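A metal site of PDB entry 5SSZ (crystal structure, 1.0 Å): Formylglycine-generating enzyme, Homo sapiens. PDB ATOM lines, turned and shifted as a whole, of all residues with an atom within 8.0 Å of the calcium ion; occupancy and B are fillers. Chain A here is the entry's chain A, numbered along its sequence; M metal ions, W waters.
O of Ile 231 touches the calcium ion, 3.9 Å away. Six residues have an atom within 4 Å of the calcium ion: Glu 67, Asn 230, Ile 231, Gly 233, Ala 235 and Glu 237. The nearest printed residue that does not touch the calcium ion is Gly 269 (4.3 Å).
The backbone carbonyl oxygen (O) of Glu 237 lies within hydrogen-bond range of the backbone NH (N) of Lys 267, 2.9 Å away. The indole nitrogen of Trp 168 lies within hydrogen-bond range of the side-chain carboxylate of Glu 237 (2.9 Å). The backbone NH (N) of Gly 233 is in hydrogen-bond range of the backbone carbonyl oxygen (O) of Gly 268 (2.9 Å). The side-chain carboxylate of Glu 67 lies within hydrogen-bond range of the side-chain amide nitrogen of Asn 234 (2.8 Å). The backbone carbonyl oxygen (O) of Asn 230 lies close to the guanidinium group (NH2) of Arg 301, at 3.4 Å. The side-chain carboxylate of Glu 237 is in salt-bridge range of the guanidinium group of Arg 301, 2.8 Å away.
The calcium ion is bound by OE2 of Glu 67 (2.3 Å). Water W1 binds the calcium ion, 2.3 Å away. O of Asn 230 is bound to the calcium ion, 2.3 Å away. The calcium ion is bound by OE2 of Glu 237 (2.4 Å). O of Ala 235 binds the calcium ion, at 2.4 Å. O of Gly 233 is bound to the calcium ion (2.4 Å).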
ATOM      1  N   TYR A  66      -4.778 -12.293 -31.523  1.00  0.00           N
ATOM      2  CA  TYR A  66      -5.630 -13.388 -31.072  1.00  0.00           C
ATOM      3  C   TYR A  66      -4.796 -14.598 -30.725  1.00  0.00           C
ATOM      4  O   TYR A  66      -3.750 -14.858 -31.336  1.00  0.00           O
ATOM      5  CB  TYR A  66      -6.583 -13.792 -32.216  1.00  0.00           C
ATOM      6  CG  TYR A  66      -7.347 -12.632 -32.816  1.00  0.00           C
ATOM      7  CD1 TYR A  66      -8.350 -11.985 -32.115  1.00  0.00           C
ATOM      8  CD2 TYR A  66      -7.051 -12.184 -34.097  1.00  0.00           C
ATOM      9  CE1 TYR A  66      -9.053 -10.924 -32.671  1.00  0.00           C
ATOM     10  CE2 TYR A  66      -7.758 -11.135 -34.665  1.00  0.00           C
ATOM     11  CZ  TYR A  66      -8.751 -10.505 -33.951  1.00  0.00           C
ATOM     12  OH  TYR A  66      -9.440  -9.460 -34.532  1.00  0.00           O
ATOM     13  N   GLU A  67      -5.287 -15.380 -29.762  1.00  0.00           N
ATOM     14  CA  GLU A  67      -4.847 -16.772 -29.639  1.00  0.00           C
ATOM     15  C   GLU A  67      -4.972 -17.451 -31.006  1.00  0.00           C
ATOM     16  O   GLU A  67      -5.893 -17.148 -31.761  1.00  0.00           O
ATOM     17  CB  GLU A  67      -5.746 -17.514 -28.650  1.00  0.00           C
ATOM     18  CG  GLU A  67      -5.671 -16.987 -27.220  1.00  0.00           C
ATOM     19  CD  GLU A  67      -6.926 -17.245 -26.385  1.00  0.00           C
ATOM     20  OE1 GLU A  67      -8.031 -17.240 -26.970  1.00  0.00           O
ATOM     21  OE2 GLU A  67      -6.793 -17.414 -25.142  1.00  0.00           O
ATOM     22  N   PRO A 142      -9.845 -20.937 -29.694  1.00  0.00           N
ATOM     23  CA  PRO A 142      -8.402 -21.205 -29.625  1.00  0.00           C
ATOM     24  C   PRO A 142      -8.132 -22.701 -29.774  1.00  0.00           C
ATOM     25  O   PRO A 142      -8.848 -23.538 -29.230  1.00  0.00           O
ATOM     26  CB  PRO A 142      -8.006 -20.720 -28.227  1.00  0.00           C
ATOM     27  CG  PRO A 142      -9.295 -20.785 -27.428  1.00  0.00           C
ATOM     28  CD  PRO A 142     -10.350 -20.357 -28.429  1.00  0.00           C
ATOM     29  N   TRP A 168       5.414 -11.093 -23.356  1.00  0.00           N
ATOM     30  CA  TRP A 168       4.017 -11.468 -23.130  1.00  0.00           C
ATOM     31  C   TRP A 168       3.407 -10.605 -22.037  1.00  0.00           C
ATOM     32  O   TRP A 168       2.315 -10.050 -22.204  1.00  0.00           O
ATOM     33  CB  TRP A 168       3.946 -12.974 -22.811  1.00  0.00           C
ATOM     34  CG  TRP A 168       2.536 -13.480 -22.795  1.00  0.00           C
ATOM     35  CD1 TRP A 168       1.904 -14.187 -23.775  1.00  0.00           C
ATOM     36  CD2 TRP A 168       1.570 -13.282 -21.752  1.00  0.00           C
ATOM     37  NE1 TRP A 168       0.601 -14.442 -23.418  1.00  0.00           N
ATOM     38  CE2 TRP A 168       0.360 -13.898 -22.183  1.00  0.00           C
ATOM     39  CE3 TRP A 168       1.599 -12.669 -20.500  1.00  0.00           C
ATOM     40  CZ2 TRP A 168      -0.794 -13.868 -21.420  1.00  0.00           C
ATOM     41  CZ3 TRP A 168       0.446 -12.643 -19.750  1.00  0.00           C
ATOM     42  CH2 TRP A 168      -0.739 -13.233 -20.215  1.00  0.00           C
ATOM     43  N   ASN A 196     -12.861 -14.412 -20.317  1.00  0.00           N
ATOM     44  CA  ASN A 196     -13.532 -15.705 -20.131  1.00  0.00           C
ATOM     45  C   ASN A 196     -12.804 -16.494 -19.057  1.00  0.00           C
ATOM     46  O   ASN A 196     -11.757 -17.112 -19.316  1.00  0.00           O
ATOM     47  CB  ASN A 196     -13.543 -16.459 -21.456  1.00  0.00           C
ATOM     48  CG  ASN A 196     -14.220 -17.798 -21.340  1.00  0.00           C
ATOM     49  OD1 ASN A 196     -14.980 -18.033 -20.387  1.00  0.00           O
ATOM     50  ND2 ASN A 196     -13.995 -18.679 -22.303  1.00  0.00           N
ATOM     51  N   TYR A 229      -6.695  -9.541 -27.672  1.00  0.00           N
ATOM     52  CA  TYR A 229      -7.898 -10.200 -27.208  1.00  0.00           C
ATOM     53  C   TYR A 229      -7.530 -11.443 -26.405  1.00  0.00           C
ATOM     54  O   TYR A 229      -6.637 -12.196 -26.773  1.00  0.00           O
ATOM     55  CB  TYR A 229      -8.766 -10.625 -28.400  1.00  0.00           C
ATOM     56  CG  TYR A 229      -9.322  -9.463 -29.168  1.00  0.00           C
ATOM     57  CD1 TYR A 229      -8.533  -8.763 -30.074  1.00  0.00           C
ATOM     58  CD2 TYR A 229     -10.635  -9.039 -28.974  1.00  0.00           C
ATOM     59  CE1 TYR A 229      -9.023  -7.686 -30.772  1.00  0.00           C
ATOM     60  CE2 TYR A 229     -11.126  -7.958 -29.658  1.00  0.00           C
ATOM     61  CZ  TYR A 229     -10.331  -7.287 -30.564  1.00  0.00           C
ATOM     62  OH  TYR A 229     -10.817  -6.199 -31.250  1.00  0.00           O
ATOM     63  N   ASN A 230      -8.261 -11.646 -25.304  1.00  0.00           N
ATOM     64  CA  ASN A 230      -8.177 -12.868 -24.497  1.00  0.00           C
ATOM     65  C   ASN A 230      -6.773 -13.165 -24.022  1.00  0.00           C
ATOM     66  O   ASN A 230      -6.401 -14.322 -23.853  1.00  0.00           O
ATOM     67  CB  ASN A 230      -8.825 -14.051 -25.206  1.00  0.00           C
ATOM     68  CG  ASN A 230     -10.271 -13.773 -25.490  1.00  0.00           C
ATOM     69  OD1 ASN A 230     -11.067 -13.634 -24.559  1.00  0.00           O
ATOM     70  ND2 ASN A 230     -10.611 -13.596 -26.756  1.00  0.00           N
ATOM     71  N   ILE A 231      -6.013 -12.109 -23.733  1.00  0.00           N
ATOM     72  CA  ILE A 231      -4.660 -12.273 -23.214  1.00  0.00           C
ATOM     73  C   ILE A 231      -4.686 -12.832 -21.806  1.00  0.00           C
ATOM     74  O   ILE A 231      -3.840 -13.654 -21.423  1.00  0.00           O
ATOM     75  CB  ILE A 231      -3.877 -10.943 -23.365  1.00  0.00           C
ATOM     76  CG1 ILE A 231      -2.366 -11.153 -23.261  1.00  0.00           C
ATOM     77  CG2 ILE A 231      -4.348  -9.897 -22.359  1.00  0.00           C
ATOM     78  CD1 ILE A 231      -1.760 -11.955 -24.384  1.00  0.00           C
ATOM     79  N   VAL A 232      -5.690 -12.437 -20.991  1.00  0.00           N
ATOM     80  CA  VAL A 232      -6.018 -13.220 -19.804  1.00  0.00           C
ATOM     81  C   VAL A 232      -7.284 -14.001 -20.074  1.00  0.00           C
ATOM     82  O   VAL A 232      -8.204 -13.538 -20.775  1.00  0.00           O
ATOM     83  CB  VAL A 232      -6.065 -12.434 -18.469  1.00  0.00           C
ATOM     84  CG1 VAL A 232      -4.734 -11.790 -18.205  1.00  0.00           C
ATOM     85  CG2 VAL A 232      -7.227 -11.434 -18.423  1.00  0.00           C
ATOM     86  N   GLY A 233      -7.349 -15.217 -19.535  1.00  0.00           N
ATOM     87  CA  GLY A 233      -8.481 -16.082 -19.730  1.00  0.00           C
ATOM     88  C   GLY A 233      -8.520 -16.770 -21.081  1.00  0.00           C
ATOM     89  O   GLY A 233      -7.623 -16.638 -21.918  1.00  0.00           O
ATOM     90  N   ASN A 234      -9.596 -17.524 -21.271  1.00  0.00           N
ATOM     91  CA  ASN A 234      -9.846 -18.294 -22.485  1.00  0.00           C
ATOM     92  C   ASN A 234      -8.894 -19.500 -22.503  1.00  0.00           C
ATOM     93  O   ASN A 234      -9.153 -20.473 -21.776  1.00  0.00           O
ATOM     94  CB  ASN A 234      -9.901 -17.437 -23.762  1.00  0.00           C
ATOM     95  CG  ASN A 234     -10.921 -17.961 -24.750  1.00  0.00           C
ATOM     96  OD1 ASN A 234     -11.942 -18.525 -24.340  1.00  0.00           O
ATOM     97  ND2 ASN A 234     -10.663 -17.762 -26.037  1.00  0.00           N
ATOM     98  N   ALA A 235      -7.809 -19.479 -23.270  1.00  0.00           N
ATOM     99  CA  ALA A 235      -6.764 -20.486 -23.148  1.00  0.00           C
ATOM    100  C   ALA A 235      -5.542 -19.882 -22.472  1.00  0.00           C
ATOM    101  O   ALA A 235      -5.178 -18.731 -22.732  1.00  0.00           O
ATOM    102  CB  ALA A 235      -6.349 -21.012 -24.536  1.00  0.00           C
ATOM    103  N   TRP A 236      -4.861 -20.684 -21.639  1.00  0.00           N
ATOM    104  CA  TRP A 236      -3.497 -20.374 -21.230  1.00  0.00           C
ATOM    105  C   TRP A 236      -2.617 -20.232 -22.465  1.00  0.00           C
ATOM    106  O   TRP A 236      -2.926 -20.767 -23.531  1.00  0.00           O
ATOM    107  CB  TRP A 236      -2.915 -21.537 -20.431  1.00  0.00           C
ATOM    108  CG  TRP A 236      -3.255 -21.590 -18.967  1.00  0.00           C
ATOM    109  CD1 TRP A 236      -4.242 -22.319 -18.367  1.00  0.00           C
ATOM    110  CD2 TRP A 236      -2.552 -20.946 -17.915  1.00  0.00           C
ATOM    111  NE1 TRP A 236      -4.195 -22.149 -17.004  1.00  0.00           N
ATOM    112  CE2 TRP A 236      -3.163 -21.313 -16.691  1.00  0.00           C
ATOM    113  CE3 TRP A 236      -1.444 -20.095 -17.878  1.00  0.00           C
ATOM    114  CZ2 TRP A 236      -2.698 -20.846 -15.452  1.00  0.00           C
ATOM    115  CZ3 TRP A 236      -0.989 -19.638 -16.659  1.00  0.00           C
ATOM    116  CH2 TRP A 236      -1.615 -20.012 -15.464  1.00  0.00           C
ATOM    117  N   GLU A 237      -1.458 -19.570 -22.305  1.00  0.00           N
ATOM    118  CA  GLU A 237      -0.603 -19.268 -23.458  1.00  0.00           C
ATOM    119  C   GLU A 237       0.849 -19.599 -23.168  1.00  0.00           C
ATOM    120  O   GLU A 237       1.451 -19.055 -22.238  1.00  0.00           O
ATOM    121  CB  GLU A 237      -0.780 -17.800 -23.873  1.00  0.00           C
ATOM    122  CG  GLU A 237      -2.251 -17.510 -24.125  1.00  0.00           C
ATOM    123  CD  GLU A 237      -2.589 -16.102 -24.551  1.00  0.00           C
ATOM    124  OE1 GLU A 237      -1.670 -15.347 -24.943  1.00  0.00           O
ATOM    125  OE2 GLU A 237      -3.806 -15.790 -24.570  1.00  0.00           O
ATOM    126  N   LYS A 267       1.335 -18.407 -19.427  1.00  0.00           N
ATOM    127  CA  LYS A 267       0.812 -17.184 -18.863  1.00  0.00           C
ATOM    128  C   LYS A 267      -0.681 -17.031 -19.126  1.00  0.00           C
ATOM    129  O   LYS A 267      -1.221 -17.557 -20.116  1.00  0.00           O
ATOM    130  CB  LYS A 267       1.524 -15.954 -19.469  1.00  0.00           C
ATOM    131  CG  LYS A 267       3.022 -15.870 -19.133  1.00  0.00           C
ATOM    132  CD  LYS A 267       3.317 -15.418 -17.705  1.00  0.00           C
ATOM    133  CE  LYS A 267       3.326 -13.890 -17.566  1.00  0.00           C
ATOM    134  NZ  LYS A 267       3.866 -13.485 -16.232  1.00  0.00           N
ATOM    135  N   GLY A 268      -1.337 -16.267 -18.261  1.00  0.00           N
ATOM    136  CA  GLY A 268      -2.594 -15.617 -18.565  1.00  0.00           C
ATOM    137  C   GLY A 268      -3.852 -16.289 -18.058  1.00  0.00           C
ATOM    138  O   GLY A 268      -4.921 -15.656 -18.059  1.00  0.00           O
ATOM    139  N   GLY A 269      -3.787 -17.549 -17.637  1.00  0.00           N
ATOM    140  CA  GLY A 269      -4.979 -18.215 -17.171  1.00  0.00           C
ATOM    141  C   GLY A 269      -5.932 -18.592 -18.307  1.00  0.00           C
ATOM    142  O   GLY A 269      -5.694 -18.357 -19.488  1.00  0.00           O
ATOM    143  N   SER A 270      -7.057 -19.191 -17.889  1.00  0.00           N
ATOM    144  CA  SER A 270      -7.970 -19.835 -18.832  1.00  0.00           C
ATOM    145  C   SER A 270      -9.411 -19.691 -18.366  1.00  0.00           C
ATOM    146  O   SER A 270      -9.705 -19.163 -17.284  1.00  0.00           O
ATOM    147  CB  SER A 270      -7.666 -21.334 -18.992  1.00  0.00           C
ATOM    148  OG  SER A 270      -8.188 -22.110 -17.923  1.00  0.00           O
ATOM    149  N   TYR A 271     -10.305 -20.272 -19.170  1.00  0.00           N
ATOM    150  CA  TYR A 271     -11.728 -20.344 -18.846  1.00  0.00           C
ATOM    151  C   TYR A 271     -12.024 -21.078 -17.545  1.00  0.00           C
ATOM    152  O   TYR A 271     -13.149 -20.955 -17.029  1.00  0.00           O
ATOM    153  CB  TYR A 271     -12.480 -20.977 -20.021  1.00  0.00           C
ATOM    154  CG  TYR A 271     -12.283 -22.467 -20.220  1.00  0.00           C
ATOM    155  CD1 TYR A 271     -12.985 -23.383 -19.451  1.00  0.00           C
ATOM    156  CD2 TYR A 271     -11.456 -22.931 -21.221  1.00  0.00           C
ATOM    157  CE1 TYR A 271     -12.846 -24.743 -19.650  1.00  0.00           C
ATOM    158  CE2 TYR A 271     -11.322 -24.315 -21.436  1.00  0.00           C
ATOM    159  CZ  TYR A 271     -12.027 -25.197 -20.632  1.00  0.00           C
ATOM    160  OH  TYR A 271     -11.929 -26.565 -20.832  1.00  0.00           O
ATOM    161  N   ASN A 297      -7.030 -26.709 -21.742  1.00  0.00           N
ATOM    162  CA  ASN A 297      -7.158 -25.279 -21.457  1.00  0.00           C
ATOM    163  C   ASN A 297      -5.908 -24.491 -21.855  1.00  0.00           C
ATOM    164  O   ASN A 297      -5.731 -23.369 -21.362  1.00  0.00           O
ATOM    165  CB  ASN A 297      -7.483 -25.030 -19.994  1.00  0.00           C
ATOM    166  CG  ASN A 297      -6.336 -25.369 -19.089  1.00  0.00           C
ATOM    167  OD1 ASN A 297      -5.375 -26.021 -19.522  1.00  0.00           O
ATOM    168  ND2 ASN A 297      -6.416 -24.951 -17.833  1.00  0.00           N
ATOM    169  N   GLY A 299      -3.284 -23.157 -24.956  1.00  0.00           N
ATOM    170  CA  GLY A 299      -3.017 -22.766 -26.319  1.00  0.00           C
ATOM    171  C   GLY A 299      -1.826 -21.818 -26.381  1.00  0.00           C
ATOM    172  O   GLY A 299      -0.873 -21.927 -25.606  1.00  0.00           O
ATOM    173  N   PHE A 300      -1.875 -20.877 -27.335  1.00  0.00           N
ATOM    174  CA  PHE A 300      -0.744 -19.974 -27.529  1.00  0.00           C
ATOM    175  C   PHE A 300      -1.114 -18.894 -28.534  1.00  0.00           C
ATOM    176  O   PHE A 300      -2.072 -19.032 -29.299  1.00  0.00           O
ATOM    177  CB  PHE A 300       0.522 -20.698 -28.017  1.00  0.00           C
ATOM    178  CG  PHE A 300       0.403 -21.294 -29.390  1.00  0.00           C
ATOM    179  CD1 PHE A 300      -0.321 -22.461 -29.597  1.00  0.00           C
ATOM    180  CD2 PHE A 300       1.027 -20.712 -30.490  1.00  0.00           C
ATOM    181  CE1 PHE A 300      -0.459 -23.021 -30.863  1.00  0.00           C
ATOM    182  CE2 PHE A 300       0.900 -21.280 -31.753  1.00  0.00           C
ATOM    183  CZ  PHE A 300       0.151 -22.424 -31.939  1.00  0.00           C
ATOM    184  N   ARG A 301      -0.281 -17.852 -28.550  1.00  0.00           N
ATOM    185  CA  ARG A 301      -0.233 -16.882 -29.643  1.00  0.00           C
ATOM    186  C   ARG A 301       1.228 -16.647 -30.019  1.00  0.00           C
ATOM    187  O   ARG A 301       2.141 -16.926 -29.241  1.00  0.00           O
ATOM    188  CB  ARG A 301      -0.927 -15.548 -29.280  1.00  0.00           C
ATOM    189  CG  ARG A 301      -0.138 -14.660 -28.327  1.00  0.00           C
ATOM    190  CD  ARG A 301      -0.901 -13.400 -27.965  1.00  0.00           C
ATOM    191  NE  ARG A 301      -2.073 -13.741 -27.169  1.00  0.00           N
ATOM    192  CZ  ARG A 301      -3.290 -13.220 -27.277  1.00  0.00           C
ATOM    193  NH1 ARG A 301      -3.573 -12.285 -28.180  1.00  0.00           N
ATOM    194  NH2 ARG A 301      -4.243 -13.639 -26.445  1.00  0.00           N
HETATM  195 CA    CA M   1      -5.682 -16.495 -23.340  1.00  0.00          CA
HETATM  196  O   HOH W   1      -4.518 -16.328 -21.325  1.00  0.00           O
